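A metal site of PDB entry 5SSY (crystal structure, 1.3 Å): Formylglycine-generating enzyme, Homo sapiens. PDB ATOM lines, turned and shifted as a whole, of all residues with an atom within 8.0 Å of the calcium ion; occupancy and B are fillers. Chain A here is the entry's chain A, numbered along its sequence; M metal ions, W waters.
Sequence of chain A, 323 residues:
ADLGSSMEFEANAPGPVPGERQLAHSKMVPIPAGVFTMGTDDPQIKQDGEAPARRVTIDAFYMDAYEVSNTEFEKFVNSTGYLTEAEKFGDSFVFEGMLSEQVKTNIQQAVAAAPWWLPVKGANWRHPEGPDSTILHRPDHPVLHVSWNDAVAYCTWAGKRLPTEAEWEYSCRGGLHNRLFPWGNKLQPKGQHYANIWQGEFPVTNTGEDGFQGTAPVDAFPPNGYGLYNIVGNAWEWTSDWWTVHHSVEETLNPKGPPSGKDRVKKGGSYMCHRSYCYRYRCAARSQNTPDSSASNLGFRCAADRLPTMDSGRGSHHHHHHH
ND2 of Asn 196 sits close to N of Ala 216 (3.5 Å). The backbone carbonyl oxygen of Asn 196 lies close to the backbone NH of Tyr 271 (3.5 Å). The side-chain amide oxygen of Asn 234 is in hydrogen-bond range of the side-chain amide nitrogen of Asn 196. ND2 of Asn 196 sits at hydrogen-bond distance from O of Gly 214 (2.9 Å). The backbone NH (N) of Asp 210 is in hydrogen-bond range of the side-chain amide oxygen (OE1) of Gln 199, at 3.0 Å. O of Ile 197 lies close to NE2 of Gln 199, at 3.4 Å.
The calcium ion is bound by O of Phe 212 (2.3 Å), O of Ile 197 (2.3 Å), water W1 (2.4 Å), OD1 of Asn 196 (2.4 Å), water W2 (2.4 Å), OD1 of Asp 210 (2.4 Å) and OD2 of Asp 210 (2.5 Å). The calcium ion has seven donor atoms within binding distance.
Water W2 lies within hydrogen-bond range of O of Tyr 271 (2.7 Å), O of Gln 213 (2.7 Å) and ND2 of Asn 206 (3.1 Å). Water W1 lies within hydrogen-bond range of OE1 of Gln 199 (2.7 Å) and OD1 of Asn 206 (2.7 Å).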
ATOM      1  N   HIS A 193      22.296 -30.164   4.610  1.00  0.00           N
ATOM      2  CA  HIS A 193      22.689 -28.793   4.879  1.00  0.00           C
ATOM      3  C   HIS A 193      23.740 -28.755   5.988  1.00  0.00           C
ATOM      4  O   HIS A 193      23.562 -29.379   7.039  1.00  0.00           O
ATOM      5  CB  HIS A 193      21.479 -27.942   5.225  1.00  0.00           C
ATOM      6  CG  HIS A 193      20.650 -27.579   4.031  1.00  0.00           C
ATOM      7  ND1 HIS A 193      21.007 -26.549   3.181  1.00  0.00           N
ATOM      8  CD2 HIS A 193      19.532 -28.126   3.513  1.00  0.00           C
ATOM      9  CE1 HIS A 193      20.122 -26.482   2.201  1.00  0.00           C
ATOM     10  NE2 HIS A 193      19.224 -27.421   2.377  1.00  0.00           N
ATOM     11  N   ALA A 195      25.262 -25.607   6.983  1.00  0.00           N
ATOM     12  CA  ALA A 195      25.355 -24.274   7.555  1.00  0.00           C
ATOM     13  C   ALA A 195      24.049 -23.542   7.325  1.00  0.00           C
ATOM     14  O   ALA A 195      23.272 -23.885   6.425  1.00  0.00           O
ATOM     15  CB  ALA A 195      26.516 -23.479   6.950  1.00  0.00           C
ATOM     16  N   ASN A 196      23.818 -22.526   8.138  1.00  0.00           N
ATOM     17  CA  ASN A 196      22.580 -21.742   8.095  1.00  0.00           C
ATOM     18  C   ASN A 196      22.820 -20.516   7.222  1.00  0.00           C
ATOM     19  O   ASN A 196      23.417 -19.535   7.678  1.00  0.00           O
ATOM     20  CB  ASN A 196      22.173 -21.325   9.496  1.00  0.00           C
ATOM     21  CG  ASN A 196      20.914 -20.475   9.511  1.00  0.00           C
ATOM     22  OD1 ASN A 196      20.175 -20.431   8.531  1.00  0.00           O
ATOM     23  ND2 ASN A 196      20.657 -19.816  10.617  1.00  0.00           N
ATOM     24  N   ILE A 197      22.378 -20.597   5.971  1.00  0.00           N
ATOM     25  CA  ILE A 197      22.404 -19.458   5.056  1.00  0.00           C
ATOM     26  C   ILE A 197      21.024 -19.288   4.437  1.00  0.00           C
ATOM     27  O   ILE A 197      20.036 -19.807   4.968  1.00  0.00           O
ATOM     28  CB  ILE A 197      23.513 -19.598   3.991  1.00  0.00           C
ATOM     29  CG1 ILE A 197      23.303 -20.852   3.132  1.00  0.00           C
ATOM     30  CG2 ILE A 197      24.886 -19.622   4.684  1.00  0.00           C
ATOM     31  CD1 ILE A 197      24.252 -20.934   1.963  1.00  0.00           C
ATOM     32  N   TRP A 198      20.915 -18.551   3.346  1.00  0.00           N
ATOM     33  CA  TRP A 198      19.608 -18.290   2.756  1.00  0.00           C
ATOM     34  C   TRP A 198      19.327 -19.289   1.639  1.00  0.00           C
ATOM     35  O   TRP A 198      20.219 -19.609   0.844  1.00  0.00           O
ATOM     36  CB  TRP A 198      19.621 -16.878   2.184  1.00  0.00           C
ATOM     37  CG  TRP A 198      18.331 -16.327   1.575  1.00  0.00           C
ATOM     38  CD1 TRP A 198      17.756 -16.671   0.388  1.00  0.00           C
ATOM     39  CD2 TRP A 198      17.521 -15.285   2.129  1.00  0.00           C
ATOM     40  NE1 TRP A 198      16.631 -15.907   0.164  1.00  0.00           N
ATOM     41  CE2 TRP A 198      16.464 -15.049   1.215  1.00  0.00           C
ATOM     42  CE3 TRP A 198      17.591 -14.529   3.301  1.00  0.00           C
ATOM     43  CZ2 TRP A 198      15.472 -14.093   1.466  1.00  0.00           C
ATOM     44  CZ3 TRP A 198      16.616 -13.589   3.534  1.00  0.00           C
ATOM     45  CH2 TRP A 198      15.571 -13.374   2.622  1.00  0.00           C
ATOM     46  N   GLN A 199      18.097 -19.786   1.591  1.00  0.00           N
ATOM     47  CA  GLN A 199      17.610 -20.486   0.407  1.00  0.00           C
ATOM     48  C   GLN A 199      16.395 -19.766  -0.163  1.00  0.00           C
ATOM     49  O   GLN A 199      15.560 -19.248   0.574  1.00  0.00           O
ATOM     50  CB  GLN A 199      17.254 -21.970   0.676  1.00  0.00           C
ATOM     51  CG  GLN A 199      18.422 -22.842   1.139  1.00  0.00           C
ATOM     52  CD  GLN A 199      18.634 -22.717   2.629  1.00  0.00           C
ATOM     53  OE1 GLN A 199      17.666 -22.660   3.393  1.00  0.00           O
ATOM     54  NE2 GLN A 199      19.891 -22.654   3.057  1.00  0.00           N
ATOM     55  N   ASN A 206      12.748 -16.451   1.619  1.00  0.00           N
ATOM     56  CA  ASN A 206      13.705 -17.343   2.278  1.00  0.00           C
ATOM     57  C   ASN A 206      12.916 -18.588   2.648  1.00  0.00           C
ATOM     58  O   ASN A 206      12.039 -18.548   3.513  1.00  0.00           O
ATOM     59  CB  ASN A 206      14.294 -16.691   3.531  1.00  0.00           C
ATOM     60  CG  ASN A 206      15.353 -17.530   4.188  1.00  0.00           C
ATOM     61  OD1 ASN A 206      15.586 -18.668   3.803  1.00  0.00           O
ATOM     62  ND2 ASN A 206      16.018 -16.975   5.177  1.00  0.00           N
ATOM     63  N   THR A 207      13.212 -19.709   1.989  1.00  0.00           N
ATOM     64  CA  THR A 207      12.337 -20.854   2.174  1.00  0.00           C
ATOM     65  C   THR A 207      12.533 -21.556   3.507  1.00  0.00           C
ATOM     66  O   THR A 207      11.669 -22.340   3.910  1.00  0.00           O
ATOM     67  CB  THR A 207      12.593 -21.889   1.080  1.00  0.00           C
ATOM     68  OG1 THR A 207      13.935 -22.375   1.240  1.00  0.00           O
ATOM     69  CG2 THR A 207      12.426 -21.282  -0.314  1.00  0.00           C
ATOM     70  N   GLY A 208      13.647 -21.308   4.180  1.00  0.00           N
ATOM     71  CA  GLY A 208      13.903 -22.033   5.398  1.00  0.00           C
ATOM     72  C   GLY A 208      14.191 -23.507   5.168  1.00  0.00           C
ATOM     73  O   GLY A 208      13.987 -24.319   6.066  1.00  0.00           O
ATOM     74  N   GLU A 209      14.641 -23.854   3.958  1.00  0.00           N
ATOM     75  CA  GLU A 209      14.943 -25.251   3.647  1.00  0.00           C
ATOM     76  C   GLU A 209      15.958 -25.842   4.624  1.00  0.00           C
ATOM     77  O   GLU A 209      15.848 -27.017   4.994  1.00  0.00           O
ATOM     78  CB  GLU A 209      15.447 -25.356   2.205  1.00  0.00           C
ATOM     79  CG  GLU A 209      15.858 -26.760   1.789  1.00  0.00           C
ATOM     80  CD  GLU A 209      16.604 -26.741   0.488  1.00  0.00           C
ATOM     81  OE1 GLU A 209      16.458 -25.759  -0.268  1.00  0.00           O
ATOM     82  OE2 GLU A 209      17.376 -27.694   0.224  1.00  0.00           O
ATOM     83  N   ASP A 210      16.944 -25.054   5.064  1.00  0.00           N
ATOM     84  CA  ASP A 210      17.961 -25.561   5.987  1.00  0.00           C
ATOM     85  C   ASP A 210      17.463 -25.678   7.430  1.00  0.00           C
ATOM     86  O   ASP A 210      18.233 -26.084   8.309  1.00  0.00           O
ATOM     87  CB  ASP A 210      19.254 -24.761   5.870  1.00  0.00           C
ATOM     88  CG  ASP A 210      19.114 -23.297   6.305  1.00  0.00           C
ATOM     89  OD1 ASP A 210      18.155 -22.947   7.049  1.00  0.00           O
ATOM     90  OD2 ASP A 210      19.974 -22.502   5.894  1.00  0.00           O
ATOM     91  N   GLY A 211      16.211 -25.319   7.685  1.00  0.00           N
ATOM     92  CA  GLY A 211      15.628 -25.439   9.000  1.00  0.00           C
ATOM     93  C   GLY A 211      15.483 -24.136   9.760  1.00  0.00           C
ATOM     94  O   GLY A 211      14.875 -24.132  10.843  1.00  0.00           O
ATOM     95  N   PHE A 212      16.013 -23.031   9.240  1.00  0.00           N
ATOM     96  CA  PHE A 212      16.058 -21.757   9.976  1.00  0.00           C
ATOM     97  C   PHE A 212      16.003 -20.589   9.016  1.00  0.00           C
ATOM     98  O   PHE A 212      16.882 -20.457   8.153  1.00  0.00           O
ATOM     99  CB  PHE A 212      17.339 -21.678  10.818  1.00  0.00           C
ATOM    100  CG  PHE A 212      17.482 -22.826  11.770  1.00  0.00           C
ATOM    101  CD1 PHE A 212      16.832 -22.807  12.984  1.00  0.00           C
ATOM    102  CD2 PHE A 212      18.209 -23.949  11.399  1.00  0.00           C
ATOM    103  CE1 PHE A 212      16.934 -23.898  13.851  1.00  0.00           C
ATOM    104  CE2 PHE A 212      18.319 -25.029  12.251  1.00  0.00           C
ATOM    105  CZ  PHE A 212      17.691 -25.004  13.481  1.00  0.00           C
ATOM    106  N   GLN A 213      14.997 -19.738   9.160  1.00  0.00           N
ATOM    107  CA  GLN A 213      14.963 -18.505   8.375  1.00  0.00           C
ATOM    108  C   GLN A 213      15.844 -17.443   9.001  1.00  0.00           C
ATOM    109  O   GLN A 213      16.650 -16.811   8.304  1.00  0.00           O
ATOM    110  CB  GLN A 213      13.521 -18.028   8.171  1.00  0.00           C
ATOM    111  CG  GLN A 213      12.752 -18.970   7.270  1.00  0.00           C
ATOM    112  CD  GLN A 213      11.271 -18.674   7.246  1.00  0.00           C
ATOM    113  OE1 GLN A 213      10.621 -18.627   8.287  1.00  0.00           O
ATOM    114  NE2 GLN A 213      10.732 -18.448   6.058  1.00  0.00           N
ATOM    115  N   GLY A 214      15.751 -17.255  10.317  1.00  0.00           N
ATOM    116  CA  GLY A 214      16.679 -16.386  11.002  1.00  0.00           C
ATOM    117  C   GLY A 214      17.833 -17.219  11.547  1.00  0.00           C
ATOM    118  O   GLY A 214      18.292 -18.159  10.883  1.00  0.00           O
ATOM    119  N   THR A 215      18.282 -16.877  12.752  1.00  0.00           N
ATOM    120  CA  THR A 215      19.351 -17.627  13.389  1.00  0.00           C
ATOM    121  C   THR A 215      18.898 -19.031  13.772  1.00  0.00           C
ATOM    122  O   THR A 215      17.703 -19.345  13.865  1.00  0.00           O
ATOM    123  CB  THR A 215      19.851 -16.908  14.637  1.00  0.00           C
ATOM    124  OG1 THR A 215      18.746 -16.666  15.511  1.00  0.00           O
ATOM    125  CG2 THR A 215      20.505 -15.591  14.286  1.00  0.00           C
ATOM    126  N   ALA A 216      19.887 -19.872  13.989  1.00  0.00           N
ATOM    127  CA  ALA A 216      19.753 -21.219  14.524  1.00  0.00           C
ATOM    128  C   ALA A 216      20.475 -21.254  15.865  1.00  0.00           C
ATOM    129  O   ALA A 216      21.325 -20.398  16.138  1.00  0.00           O
ATOM    130  CB  ALA A 216      20.466 -22.194  13.573  1.00  0.00           C
ATOM    131  N   PHE A 221      23.793 -27.745  13.324  1.00  0.00           N
ATOM    132  CA  PHE A 221      24.569 -28.144  12.154  1.00  0.00           C
ATOM    133  C   PHE A 221      25.831 -28.906  12.546  1.00  0.00           C
ATOM    134  O   PHE A 221      26.213 -28.924  13.727  1.00  0.00           O
ATOM    135  CB  PHE A 221      24.823 -26.950  11.234  1.00  0.00           C
ATOM    136  CG  PHE A 221      23.564 -26.406  10.608  1.00  0.00           C
ATOM    137  CD1 PHE A 221      23.004 -27.030   9.505  1.00  0.00           C
ATOM    138  CD2 PHE A 221      22.931 -25.300  11.152  1.00  0.00           C
ATOM    139  CE1 PHE A 221      21.823 -26.561   8.954  1.00  0.00           C
ATOM    140  CE2 PHE A 221      21.764 -24.822  10.616  1.00  0.00           C
ATOM    141  CZ  PHE A 221      21.215 -25.442   9.521  1.00  0.00           C
ATOM    142  N   ASN A 234      25.005 -18.541   9.915  1.00  0.00           N
ATOM    143  CA  ASN A 234      24.379 -18.156  11.163  1.00  0.00           C
ATOM    144  C   ASN A 234      24.646 -16.670  11.449  1.00  0.00           C
ATOM    145  O   ASN A 234      24.036 -15.817  10.809  1.00  0.00           O
ATOM    146  CB  ASN A 234      24.770 -19.080  12.315  1.00  0.00           C
ATOM    147  CG  ASN A 234      23.610 -19.366  13.241  1.00  0.00           C
ATOM    148  OD1 ASN A 234      22.451 -19.335  12.829  1.00  0.00           O
ATOM    149  ND2 ASN A 234      23.913 -19.650  14.497  1.00  0.00           N
ATOM    150  N   SER A 270      26.513 -15.283   7.059  1.00  0.00           N
ATOM    151  CA  SER A 270      25.395 -15.338   7.988  1.00  0.00           C
ATOM    152  C   SER A 270      24.197 -16.038   7.345  1.00  0.00           C
ATOM    153  O   SER A 270      24.229 -16.459   6.181  1.00  0.00           O
ATOM    154  CB  SER A 270      24.976 -13.945   8.432  1.00  0.00           C
ATOM    155  OG  SER A 270      24.312 -13.264   7.387  1.00  0.00           O
ATOM    156  N   TYR A 271      23.116 -16.123   8.130  1.00  0.00           N
ATOM    157  CA  TYR A 271      21.844 -16.673   7.669  1.00  0.00           C
ATOM    158  C   TYR A 271      21.251 -15.896   6.503  1.00  0.00           C
ATOM    159  O   TYR A 271      20.275 -16.372   5.908  1.00  0.00           O
ATOM    160  CB  TYR A 271      20.807 -16.762   8.807  1.00  0.00           C
ATOM    161  CG  TYR A 271      20.362 -15.445   9.438  1.00  0.00           C
ATOM    162  CD1 TYR A 271      19.287 -14.720   8.930  1.00  0.00           C
ATOM    163  CD2 TYR A 271      21.023 -14.916  10.543  1.00  0.00           C
ATOM    164  CE1 TYR A 271      18.888 -13.505   9.516  1.00  0.00           C
ATOM    165  CE2 TYR A 271      20.634 -13.729  11.124  1.00  0.00           C
ATOM    166  CZ  TYR A 271      19.568 -13.032  10.612  1.00  0.00           C
ATOM    167  OH  TYR A 271      19.190 -11.843  11.201  1.00  0.00           O
ATOM    168  N   MET A 272      21.803 -14.742   6.175  1.00  0.00           N
ATOM    169  CA  MET A 272      21.304 -13.970   5.039  1.00  0.00           C
ATOM    170  C   MET A 272      22.034 -14.264   3.751  1.00  0.00           C
ATOM    171  O   MET A 272      21.539 -13.892   2.678  1.00  0.00           O
ATOM    172  CB  MET A 272      21.416 -12.481   5.331  1.00  0.00           C
ATOM    173  CG  MET A 272      20.423 -11.991   6.340  1.00  0.00           C
ATOM    174  SD  MET A 272      20.699 -10.271   6.725  1.00  0.00           S
ATOM    175  CE  MET A 272      20.368  -9.497   5.134  1.00  0.00           C
ATOM    176  N   CYS A 273      23.178 -14.940   3.792  1.00  0.00           N
ATOM    177  CA  CYS A 273      24.010 -15.085   2.610  1.00  0.00           C
ATOM    178  C   CYS A 273      23.378 -15.986   1.562  1.00  0.00           C
ATOM    179  O   CYS A 273      22.743 -16.992   1.873  1.00  0.00           O
ATOM    180  CB  CYS A 273      25.370 -15.667   2.977  1.00  0.00           C
ATOM    181  SG  CYS A 273      26.542 -14.497   3.742  1.00  0.00           S
HETATM  182 CA    CA M   1      18.656 -20.586   6.698  1.00  0.00          CA
HETATM  183  O   HOH W   1      17.005 -20.652   5.011  1.00  0.00           O
HETATM  184  O   HOH W   2      18.396 -18.168   6.702  1.00  0.00           O
